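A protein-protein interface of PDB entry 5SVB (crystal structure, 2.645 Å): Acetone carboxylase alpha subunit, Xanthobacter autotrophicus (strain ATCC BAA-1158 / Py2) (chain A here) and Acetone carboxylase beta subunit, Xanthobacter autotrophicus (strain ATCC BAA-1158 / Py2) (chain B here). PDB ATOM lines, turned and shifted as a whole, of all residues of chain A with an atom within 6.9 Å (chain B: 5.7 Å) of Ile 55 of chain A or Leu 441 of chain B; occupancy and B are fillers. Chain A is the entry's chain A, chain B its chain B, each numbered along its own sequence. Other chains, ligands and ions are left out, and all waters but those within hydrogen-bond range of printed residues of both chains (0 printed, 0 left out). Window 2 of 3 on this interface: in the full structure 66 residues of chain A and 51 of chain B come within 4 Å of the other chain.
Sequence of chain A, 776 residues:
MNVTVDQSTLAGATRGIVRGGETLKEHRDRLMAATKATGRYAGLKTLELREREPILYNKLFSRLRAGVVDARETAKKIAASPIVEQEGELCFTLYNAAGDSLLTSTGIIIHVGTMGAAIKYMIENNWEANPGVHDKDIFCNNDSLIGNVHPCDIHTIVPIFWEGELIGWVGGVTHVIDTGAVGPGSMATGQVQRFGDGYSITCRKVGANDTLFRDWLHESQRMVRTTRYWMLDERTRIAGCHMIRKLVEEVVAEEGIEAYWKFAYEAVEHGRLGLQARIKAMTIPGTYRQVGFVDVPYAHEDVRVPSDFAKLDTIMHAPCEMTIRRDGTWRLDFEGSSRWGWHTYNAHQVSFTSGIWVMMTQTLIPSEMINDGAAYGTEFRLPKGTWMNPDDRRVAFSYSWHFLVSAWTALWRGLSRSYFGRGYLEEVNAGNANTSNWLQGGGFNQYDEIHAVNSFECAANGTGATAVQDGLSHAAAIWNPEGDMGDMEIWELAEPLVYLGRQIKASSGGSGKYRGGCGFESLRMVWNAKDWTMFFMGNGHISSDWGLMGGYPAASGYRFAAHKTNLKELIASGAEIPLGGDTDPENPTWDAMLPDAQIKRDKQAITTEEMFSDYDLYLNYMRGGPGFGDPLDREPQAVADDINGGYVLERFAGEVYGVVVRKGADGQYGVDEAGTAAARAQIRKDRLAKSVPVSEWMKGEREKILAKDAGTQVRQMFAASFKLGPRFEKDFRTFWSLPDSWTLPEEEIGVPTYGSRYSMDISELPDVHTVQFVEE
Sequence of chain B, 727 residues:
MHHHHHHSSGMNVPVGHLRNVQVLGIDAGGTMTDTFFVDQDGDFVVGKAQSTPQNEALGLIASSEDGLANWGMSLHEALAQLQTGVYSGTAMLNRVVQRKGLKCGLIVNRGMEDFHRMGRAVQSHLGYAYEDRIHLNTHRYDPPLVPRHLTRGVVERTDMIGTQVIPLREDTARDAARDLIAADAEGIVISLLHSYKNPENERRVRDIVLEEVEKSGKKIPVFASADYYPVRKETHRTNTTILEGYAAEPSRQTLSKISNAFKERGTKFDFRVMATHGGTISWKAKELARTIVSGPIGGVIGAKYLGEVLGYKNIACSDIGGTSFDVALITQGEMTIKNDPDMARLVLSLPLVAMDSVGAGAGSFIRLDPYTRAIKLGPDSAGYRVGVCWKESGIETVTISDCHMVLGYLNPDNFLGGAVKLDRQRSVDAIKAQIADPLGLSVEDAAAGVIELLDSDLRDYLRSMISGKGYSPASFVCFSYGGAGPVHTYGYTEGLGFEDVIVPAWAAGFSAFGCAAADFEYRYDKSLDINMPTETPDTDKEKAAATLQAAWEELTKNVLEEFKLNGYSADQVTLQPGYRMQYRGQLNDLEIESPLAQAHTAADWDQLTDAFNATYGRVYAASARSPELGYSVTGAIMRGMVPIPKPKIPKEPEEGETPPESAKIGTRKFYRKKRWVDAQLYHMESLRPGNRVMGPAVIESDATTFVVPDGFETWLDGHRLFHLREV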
ATOM      1  N   LEU A  49     -28.063 -18.253  -5.008  1.00  0.00           N
ATOM      2  CA  LEU A  49     -26.702 -17.737  -5.114  1.00  0.00           C
ATOM      3  C   LEU A  49     -25.827 -18.260  -3.982  1.00  0.00           C
ATOM      4  O   LEU A  49     -24.691 -18.694  -4.208  1.00  0.00           O
ATOM      5  CB  LEU A  49     -26.725 -16.209  -5.118  1.00  0.00           C
ATOM      6  CG  LEU A  49     -25.373 -15.505  -5.233  1.00  0.00           C
ATOM      7  CD1 LEU A  49     -24.714 -15.822  -6.556  1.00  0.00           C
ATOM      8  CD2 LEU A  49     -25.555 -14.011  -5.073  1.00  0.00           C
ATOM      9  N   ARG A  50     -26.343 -18.234  -2.753  1.00  0.00           N
ATOM     10  CA  ARG A  50     -25.543 -18.655  -1.606  1.00  0.00           C
ATOM     11  C   ARG A  50     -25.232 -20.145  -1.660  1.00  0.00           C
ATOM     12  O   ARG A  50     -24.138 -20.568  -1.273  1.00  0.00           O
ATOM     13  CB  ARG A  50     -26.271 -18.313  -0.307  1.00  0.00           C
ATOM     14  CG  ARG A  50     -25.468 -18.616   0.947  1.00  0.00           C
ATOM     15  CD  ARG A  50     -26.240 -18.256   2.199  1.00  0.00           C
ATOM     16  NE  ARG A  50     -27.251 -19.262   2.531  1.00  0.00           N
ATOM     17  CZ  ARG A  50     -27.358 -19.891   3.698  1.00  0.00           C
ATOM     18  NH1 ARG A  50     -26.527 -19.632   4.698  1.00  0.00           N
ATOM     19  NH2 ARG A  50     -28.320 -20.787   3.875  1.00  0.00           N
ATOM     20  N   GLU A  51     -26.178 -20.954  -2.129  1.00  0.00           N
ATOM     21  CA  GLU A  51     -26.020 -22.403  -2.107  1.00  0.00           C
ATOM     22  C   GLU A  51     -25.301 -22.945  -3.335  1.00  0.00           C
ATOM     23  O   GLU A  51     -24.563 -23.929  -3.225  1.00  0.00           O
ATOM     24  CB  GLU A  51     -27.391 -23.071  -1.982  1.00  0.00           C
ATOM     25  CG  GLU A  51     -28.157 -22.662  -0.734  1.00  0.00           C
ATOM     26  CD  GLU A  51     -29.636 -22.974  -0.829  1.00  0.00           C
ATOM     27  OE1 GLU A  51     -30.007 -23.855  -1.635  1.00  0.00           O
ATOM     28  OE2 GLU A  51     -30.428 -22.333  -0.105  1.00  0.00           O
ATOM     29  N   ARG A  52     -25.493 -22.329  -4.499  1.00  0.00           N
ATOM     30  CA  ARG A  52     -24.880 -22.806  -5.730  1.00  0.00           C
ATOM     31  C   ARG A  52     -23.591 -22.079  -6.087  1.00  0.00           C
ATOM     32  O   ARG A  52     -22.783 -22.627  -6.843  1.00  0.00           O
ATOM     33  CB  ARG A  52     -25.868 -22.669  -6.893  1.00  0.00           C
ATOM     34  CG  ARG A  52     -27.027 -23.656  -6.835  1.00  0.00           C
ATOM     35  CD  ARG A  52     -28.281 -23.099  -7.490  1.00  0.00           C
ATOM     36  NE  ARG A  52     -28.694 -23.870  -8.659  1.00  0.00           N
ATOM     37  CZ  ARG A  52     -29.722 -23.546  -9.437  1.00  0.00           C
ATOM     38  NH1 ARG A  52     -30.443 -22.462  -9.177  1.00  0.00           N
ATOM     39  NH2 ARG A  52     -30.030 -24.305 -10.481  1.00  0.00           N
ATOM     40  N   GLU A  53     -23.379 -20.869  -5.572  1.00  0.00           N
ATOM     41  CA  GLU A  53     -22.162 -20.100  -5.836  1.00  0.00           C
ATOM     42  C   GLU A  53     -21.624 -19.525  -4.530  1.00  0.00           C
ATOM     43  O   GLU A  53     -21.441 -18.313  -4.393  1.00  0.00           O
ATOM     44  CB  GLU A  53     -22.437 -18.993  -6.851  1.00  0.00           C
ATOM     45  CG  GLU A  53     -23.222 -19.455  -8.071  1.00  0.00           C
ATOM     46  CD  GLU A  53     -23.382 -18.365  -9.111  1.00  0.00           C
ATOM     47  OE1 GLU A  53     -22.362 -17.763  -9.505  1.00  0.00           O
ATOM     48  OE2 GLU A  53     -24.531 -18.105  -9.530  1.00  0.00           O
ATOM     49  N   PRO A  54     -21.345 -20.383  -3.546  1.00  0.00           N
ATOM     50  CA  PRO A  54     -20.949 -19.872  -2.220  1.00  0.00           C
ATOM     51  C   PRO A  54     -19.770 -18.913  -2.244  1.00  0.00           C
ATOM     52  O   PRO A  54     -19.836 -17.846  -1.622  1.00  0.00           O
ATOM     53  CB  PRO A  54     -20.633 -21.157  -1.439  1.00  0.00           C
ATOM     54  CG  PRO A  54     -20.467 -22.228  -2.467  1.00  0.00           C
ATOM     55  CD  PRO A  54     -21.366 -21.852  -3.589  1.00  0.00           C
ATOM     56  N   ILE A  55     -18.684 -19.260  -2.936  1.00  0.00           N
ATOM     57  CA  ILE A  55     -17.514 -18.384  -2.967  1.00  0.00           C
ATOM     58  C   ILE A  55     -17.905 -17.001  -3.475  1.00  0.00           C
ATOM     59  O   ILE A  55     -17.585 -15.980  -2.856  1.00  0.00           O
ATOM     60  CB  ILE A  55     -16.396 -19.011  -3.821  1.00  0.00           C
ATOM     61  CG1 ILE A  55     -15.572 -19.993  -2.985  1.00  0.00           C
ATOM     62  CG2 ILE A  55     -15.456 -17.946  -4.381  1.00  0.00           C
ATOM     63  CD1 ILE A  55     -16.378 -21.024  -2.240  1.00  0.00           C
ATOM     64  N   LEU A  56     -18.604 -16.948  -4.611  1.00  0.00           N
ATOM     65  CA  LEU A  56     -19.040 -15.664  -5.148  1.00  0.00           C
ATOM     66  C   LEU A  56     -19.946 -14.936  -4.165  1.00  0.00           C
ATOM     67  O   LEU A  56     -19.908 -13.705  -4.066  1.00  0.00           O
ATOM     68  CB  LEU A  56     -19.756 -15.870  -6.482  1.00  0.00           C
ATOM     69  CG  LEU A  56     -20.474 -14.645  -7.054  1.00  0.00           C
ATOM     70  CD1 LEU A  56     -19.509 -13.487  -7.257  1.00  0.00           C
ATOM     71  CD2 LEU A  56     -21.161 -15.003  -8.357  1.00  0.00           C
ATOM     72  N   TYR A  57     -20.770 -15.680  -3.427  1.00  0.00           N
ATOM     73  CA  TYR A  57     -21.662 -15.056  -2.458  1.00  0.00           C
ATOM     74  C   TYR A  57     -20.874 -14.458  -1.299  1.00  0.00           C
ATOM     75  O   TYR A  57     -21.058 -13.287  -0.947  1.00  0.00           O
ATOM     76  CB  TYR A  57     -22.676 -16.078  -1.954  1.00  0.00           C
ATOM     77  CG  TYR A  57     -23.719 -15.499  -1.035  1.00  0.00           C
ATOM     78  CD1 TYR A  57     -24.861 -14.903  -1.547  1.00  0.00           C
ATOM     79  CD2 TYR A  57     -23.566 -15.550   0.342  1.00  0.00           C
ATOM     80  CE1 TYR A  57     -25.820 -14.373  -0.717  1.00  0.00           C
ATOM     81  CE2 TYR A  57     -24.523 -15.022   1.185  1.00  0.00           C
ATOM     82  CZ  TYR A  57     -25.647 -14.435   0.647  1.00  0.00           C
ATOM     83  OH  TYR A  57     -26.609 -13.904   1.469  1.00  0.00           O
ATOM     84  N   ASN A  58     -19.991 -15.251  -0.690  1.00  0.00           N
ATOM     85  CA  ASN A  58     -19.141 -14.730   0.375  1.00  0.00           C
ATOM     86  C   ASN A  58     -18.243 -13.611  -0.130  1.00  0.00           C
ATOM     87  O   ASN A  58     -17.851 -12.731   0.645  1.00  0.00           O
ATOM     88  CB  ASN A  58     -18.298 -15.855   0.971  1.00  0.00           C
ATOM     89  CG  ASN A  58     -19.090 -16.749   1.899  1.00  0.00           C
ATOM     90  OD1 ASN A  58     -19.108 -16.541   3.110  1.00  0.00           O
ATOM     91  ND2 ASN A  58     -19.751 -17.750   1.336  1.00  0.00           N
ATOM     92  N   LYS A  59     -17.906 -13.626  -1.419  1.00  0.00           N
ATOM     93  CA  LYS A  59     -17.039 -12.591  -1.966  1.00  0.00           C
ATOM     94  C   LYS A  59     -17.768 -11.259  -2.072  1.00  0.00           C
ATOM     95  O   LYS A  59     -17.208 -10.210  -1.735  1.00  0.00           O
ATOM     96  CB  LYS A  59     -16.509 -13.029  -3.329  1.00  0.00           C
ATOM     97  CG  LYS A  59     -15.587 -12.016  -3.987  1.00  0.00           C
ATOM     98  CD  LYS A  59     -14.459 -12.682  -4.763  1.00  0.00           C
ATOM     99  CE  LYS A  59     -14.449 -12.250  -6.212  1.00  0.00           C
ATOM    100  NZ  LYS A  59     -13.193 -12.663  -6.893  1.00  0.00           N
ATOM    101  N   LEU A  60     -19.017 -11.276  -2.538  1.00  0.00           N
ATOM    102  CA  LEU A  60     -19.782 -10.038  -2.640  1.00  0.00           C
ATOM    103  C   LEU A  60     -19.938  -9.382  -1.277  1.00  0.00           C
ATOM    104  O   LEU A  60     -19.695  -8.181  -1.122  1.00  0.00           O
ATOM    105  CB  LEU A  60     -21.148 -10.312  -3.263  1.00  0.00           C
ATOM    106  CG  LEU A  60     -21.146 -10.771  -4.719  1.00  0.00           C
ATOM    107  CD1 LEU A  60     -22.532 -11.237  -5.111  1.00  0.00           C
ATOM    108  CD2 LEU A  60     -20.674  -9.660  -5.641  1.00  0.00           C
ATOM    109  N   ILE B 375     -17.865 -17.935   5.286  1.00  0.00           N
ATOM    110  CA  ILE B 375     -16.454 -18.262   5.447  1.00  0.00           C
ATOM    111  C   ILE B 375     -15.784 -17.170   6.270  1.00  0.00           C
ATOM    112  O   ILE B 375     -15.856 -15.984   5.927  1.00  0.00           O
ATOM    113  CB  ILE B 375     -15.778 -18.425   4.076  1.00  0.00           C
ATOM    114  CG1 ILE B 375     -16.491 -19.510   3.263  1.00  0.00           C
ATOM    115  CG2 ILE B 375     -14.314 -18.788   4.244  1.00  0.00           C
ATOM    116  CD1 ILE B 375     -16.186 -19.467   1.786  1.00  0.00           C
ATOM    117  N   ALA B 436     -15.375 -27.894   2.547  1.00  0.00           N
ATOM    118  CA  ALA B 436     -15.867 -28.296   1.233  1.00  0.00           C
ATOM    119  C   ALA B 436     -17.245 -28.942   1.322  1.00  0.00           C
ATOM    120  O   ALA B 436     -18.223 -28.432   0.762  1.00  0.00           O
ATOM    121  CB  ALA B 436     -14.866 -29.244   0.577  1.00  0.00           C
ATOM    122  N   ASP B 437     -17.343 -30.078   2.010  1.00  0.00           N
ATOM    123  CA  ASP B 437     -18.617 -30.788   2.103  1.00  0.00           C
ATOM    124  C   ASP B 437     -19.754 -29.905   2.599  1.00  0.00           C
ATOM    125  O   ASP B 437     -20.818 -29.895   1.961  1.00  0.00           O
ATOM    126  CB  ASP B 437     -18.448 -32.024   2.998  1.00  0.00           C
ATOM    127  CG  ASP B 437     -17.747 -33.164   2.288  1.00  0.00           C
ATOM    128  OD1 ASP B 437     -17.103 -32.912   1.249  1.00  0.00           O
ATOM    129  OD2 ASP B 437     -17.838 -34.311   2.772  1.00  0.00           O
ATOM    130  N   LEU B 439     -20.263 -26.811   2.188  1.00  0.00           N
ATOM    131  CA  LEU B 439     -20.626 -25.909   1.104  1.00  0.00           C
ATOM    132  C   LEU B 439     -21.046 -26.640  -0.164  1.00  0.00           C
ATOM    133  O   LEU B 439     -21.598 -26.006  -1.070  1.00  0.00           O
ATOM    134  CB  LEU B 439     -19.452 -24.982   0.780  1.00  0.00           C
ATOM    135  CG  LEU B 439     -18.935 -24.122   1.932  1.00  0.00           C
ATOM    136  CD1 LEU B 439     -17.676 -23.383   1.519  1.00  0.00           C
ATOM    137  CD2 LEU B 439     -19.999 -23.144   2.390  1.00  0.00           C
ATOM    138  N   GLY B 440     -20.804 -27.945  -0.253  1.00  0.00           N
ATOM    139  CA  GLY B 440     -21.118 -28.677  -1.462  1.00  0.00           C
ATOM    140  C   GLY B 440     -20.088 -28.520  -2.554  1.00  0.00           C
ATOM    141  O   GLY B 440     -20.437 -28.568  -3.737  1.00  0.00           O
ATOM    142  N   LEU B 441     -18.824 -28.334  -2.191  1.00  0.00           N
ATOM    143  CA  LEU B 441     -17.750 -28.114  -3.144  1.00  0.00           C
ATOM    144  C   LEU B 441     -16.749 -29.254  -3.065  1.00  0.00           C
ATOM    145  O   LEU B 441     -16.690 -29.993  -2.079  1.00  0.00           O
ATOM    146  CB  LEU B 441     -17.027 -26.789  -2.869  1.00  0.00           C
ATOM    147  CG  LEU B 441     -17.878 -25.522  -2.856  1.00  0.00           C
ATOM    148  CD1 LEU B 441     -17.082 -24.382  -2.254  1.00  0.00           C
ATOM    149  CD2 LEU B 441     -18.334 -25.174  -4.253  1.00  0.00           C
ATOM    150  N   SER B 442     -15.959 -29.393  -4.124  1.00  0.00           N
ATOM    151  CA  SER B 442     -14.792 -30.253  -4.055  1.00  0.00           C
ATOM    152  C   SER B 442     -13.752 -29.625  -3.136  1.00  0.00           C
ATOM    153  O   SER B 442     -13.788 -28.428  -2.840  1.00  0.00           O
ATOM    154  CB  SER B 442     -14.206 -30.477  -5.447  1.00  0.00           C
ATOM    155  OG  SER B 442     -13.771 -29.257  -6.017  1.00  0.00           O
ATOM    156  N   VAL B 443     -12.817 -30.454  -2.670  1.00  0.00           N
ATOM    157  CA  VAL B 443     -11.795 -29.964  -1.750  1.00  0.00           C
ATOM    158  C   VAL B 443     -10.952 -28.888  -2.419  1.00  0.00           C
ATOM    159  O   VAL B 443     -10.596 -27.880  -1.798  1.00  0.00           O
ATOM    160  CB  VAL B 443     -10.928 -31.132  -1.246  1.00  0.00           C
ATOM    161  CG1 VAL B 443      -9.837 -30.628  -0.319  1.00  0.00           C
ATOM    162  CG2 VAL B 443     -11.789 -32.154  -0.530  1.00  0.00           C
ATOM    163  N   ASP B 445     -11.744 -26.844  -5.027  1.00  0.00           N
ATOM    164  CA  ASP B 445     -12.500 -25.613  -5.236  1.00  0.00           C
ATOM    165  C   ASP B 445     -12.698 -24.862  -3.927  1.00  0.00           C
ATOM    166  O   ASP B 445     -12.663 -23.626  -3.900  1.00  0.00           O
ATOM    167  CB  ASP B 445     -13.849 -25.929  -5.881  1.00  0.00           C
ATOM    168  CG  ASP B 445     -13.735 -26.219  -7.363  1.00  0.00           C
ATOM    169  OD1 ASP B 445     -12.866 -25.617  -8.025  1.00  0.00           O
ATOM    170  OD2 ASP B 445     -14.519 -27.047  -7.867  1.00  0.00           O
ATOM    171  N   ALA B 446     -12.914 -25.589  -2.830  1.00  0.00           N
ATOM    172  CA  ALA B 446     -13.042 -24.941  -1.531  1.00  0.00           C
ATOM    173  C   ALA B 446     -11.753 -24.225  -1.157  1.00  0.00           C
ATOM    174  O   ALA B 446     -11.763 -23.039  -0.815  1.00  0.00           O
ATOM    175  CB  ALA B 446     -13.415 -25.971  -0.465  1.00  0.00           C
ATOM    176  N   GLY B 449     -11.119 -21.412  -3.407  1.00  0.00           N
ATOM    177  CA  GLY B 449     -12.043 -20.333  -3.105  1.00  0.00           C
ATOM    178  C   GLY B 449     -11.580 -19.477  -1.942  1.00  0.00           C
ATOM    179  O   GLY B 449     -11.643 -18.248  -2.003  1.00  0.00           O
ATOM    180  N   VAL B 450     -11.119 -20.112  -0.864  1.00  0.00           N
ATOM    181  CA  VAL B 450     -10.587 -19.359   0.268  1.00  0.00           C
ATOM    182  C   VAL B 450      -9.461 -18.446  -0.195  1.00  0.00           C
ATOM    183  O   VAL B 450      -9.432 -17.253   0.126  1.00  0.00           O
ATOM    184  CB  VAL B 450     -10.113 -20.316   1.375  1.00  0.00           C
ATOM    185  CG1 VAL B 450      -9.445 -19.542   2.500  1.00  0.00           C
ATOM    186  CG2 VAL B 450     -11.281 -21.121   1.912  1.00  0.00           C
ATOM    187  N   GLU B 452      -9.040 -17.335  -3.081  1.00  0.00           N
ATOM    188  CA  GLU B 452      -9.663 -16.288  -3.883  1.00  0.00           C
ATOM    189  C   GLU B 452     -10.223 -15.186  -2.991  1.00  0.00           C
ATOM    190  O   GLU B 452     -10.027 -13.995  -3.258  1.00  0.00           O
ATOM    191  CB  GLU B 452     -10.760 -16.887  -4.762  1.00  0.00           C
ATOM    192  CG  GLU B 452     -11.372 -15.901  -5.741  1.00  0.00           C
ATOM    193  CD  GLU B 452     -12.473 -16.519  -6.577  1.00  0.00           C
ATOM    194  OE1 GLU B 452     -12.503 -17.763  -6.695  1.00  0.00           O
ATOM    195  OE2 GLU B 452     -13.308 -15.761  -7.113  1.00  0.00           O
ATOM    196  N   LEU B 453     -10.919 -15.567  -1.918  1.00  0.00           N
ATOM    197  CA  LEU B 453     -11.436 -14.574  -0.983  1.00  0.00           C
ATOM    198  C   LEU B 453     -10.306 -13.738  -0.401  1.00  0.00           C
ATOM    199  O   LEU B 453     -10.384 -12.505  -0.364  1.00  0.00           O
ATOM    200  CB  LEU B 453     -12.217 -15.264   0.135  1.00  0.00           C
ATOM    201  CG  LEU B 453     -13.440 -16.079  -0.286  1.00  0.00           C
ATOM    202  CD1 LEU B 453     -14.027 -16.803   0.909  1.00  0.00           C
ATOM    203  CD2 LEU B 453     -14.485 -15.196  -0.932  1.00  0.00           C
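The backbone NH (N) of Ile 375 of chain B sits at hydrogen-bond distance from the side-chain amide oxygen (OD1) of Asn 58 of chain A (2.9 Å). OE2 of Glu 452 of chain B is in salt-bridge range of NZ of Lys 59 of chain A.
O of Pro 54 of chain A sits at hydrogen-bond distance from ND2 of Asn 58 of chain A, at 3.0 Å. N of Leu 441 of chain B lies within hydrogen-bond range of O of Ala 436 of chain B, at 3.0 Å.
Leu 441 of chain B touches Ile 55 of chain A. Gly 449 of chain B touches Ile 55 of chain A. Glu 452 of chain B touches Ile 55 of chain A. Leu 453 of chain B touches Ile 55 of chain A (CD2 to O, 3.7 Å). CA of Lys 59 of chain A touches CD2 of Leu 453 of chain B (3.8 Å).
Ile 55 of chain A touches four residues of chain B. Of the printed residues of chain A, Leu 441 of chain B touches Ile 55. Gly 440 of chain B touches none of the printed residues of chain A. Printed residues of chain B within 4 Å of Lys 59 of chain A: Glu 452 and Leu 453. Printed residues of chain A within 4 Å of Ile 375 of chain B: Asn 58 (2.9 Å). Val 450 of chain B touches none of the printed residues of chain A. The nearest residue of chain B that does not touch Ile 55 of chain A is Ile 375 of chain B (4.3 Å). The nearest printed residue of chain A that does not touch Leu 441 of chain B is Pro 54 of chain A (4.02 Å).
Of the 12 printed residues of chain A, 3 touch a printed residue of chain B. Hydrophobic or aromatic side chains of chain A within 4 Å of the printed part of chain B: Ile 55. Along chain A the printed residues that touch a printed residue of chain B span positions 55 to 59.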
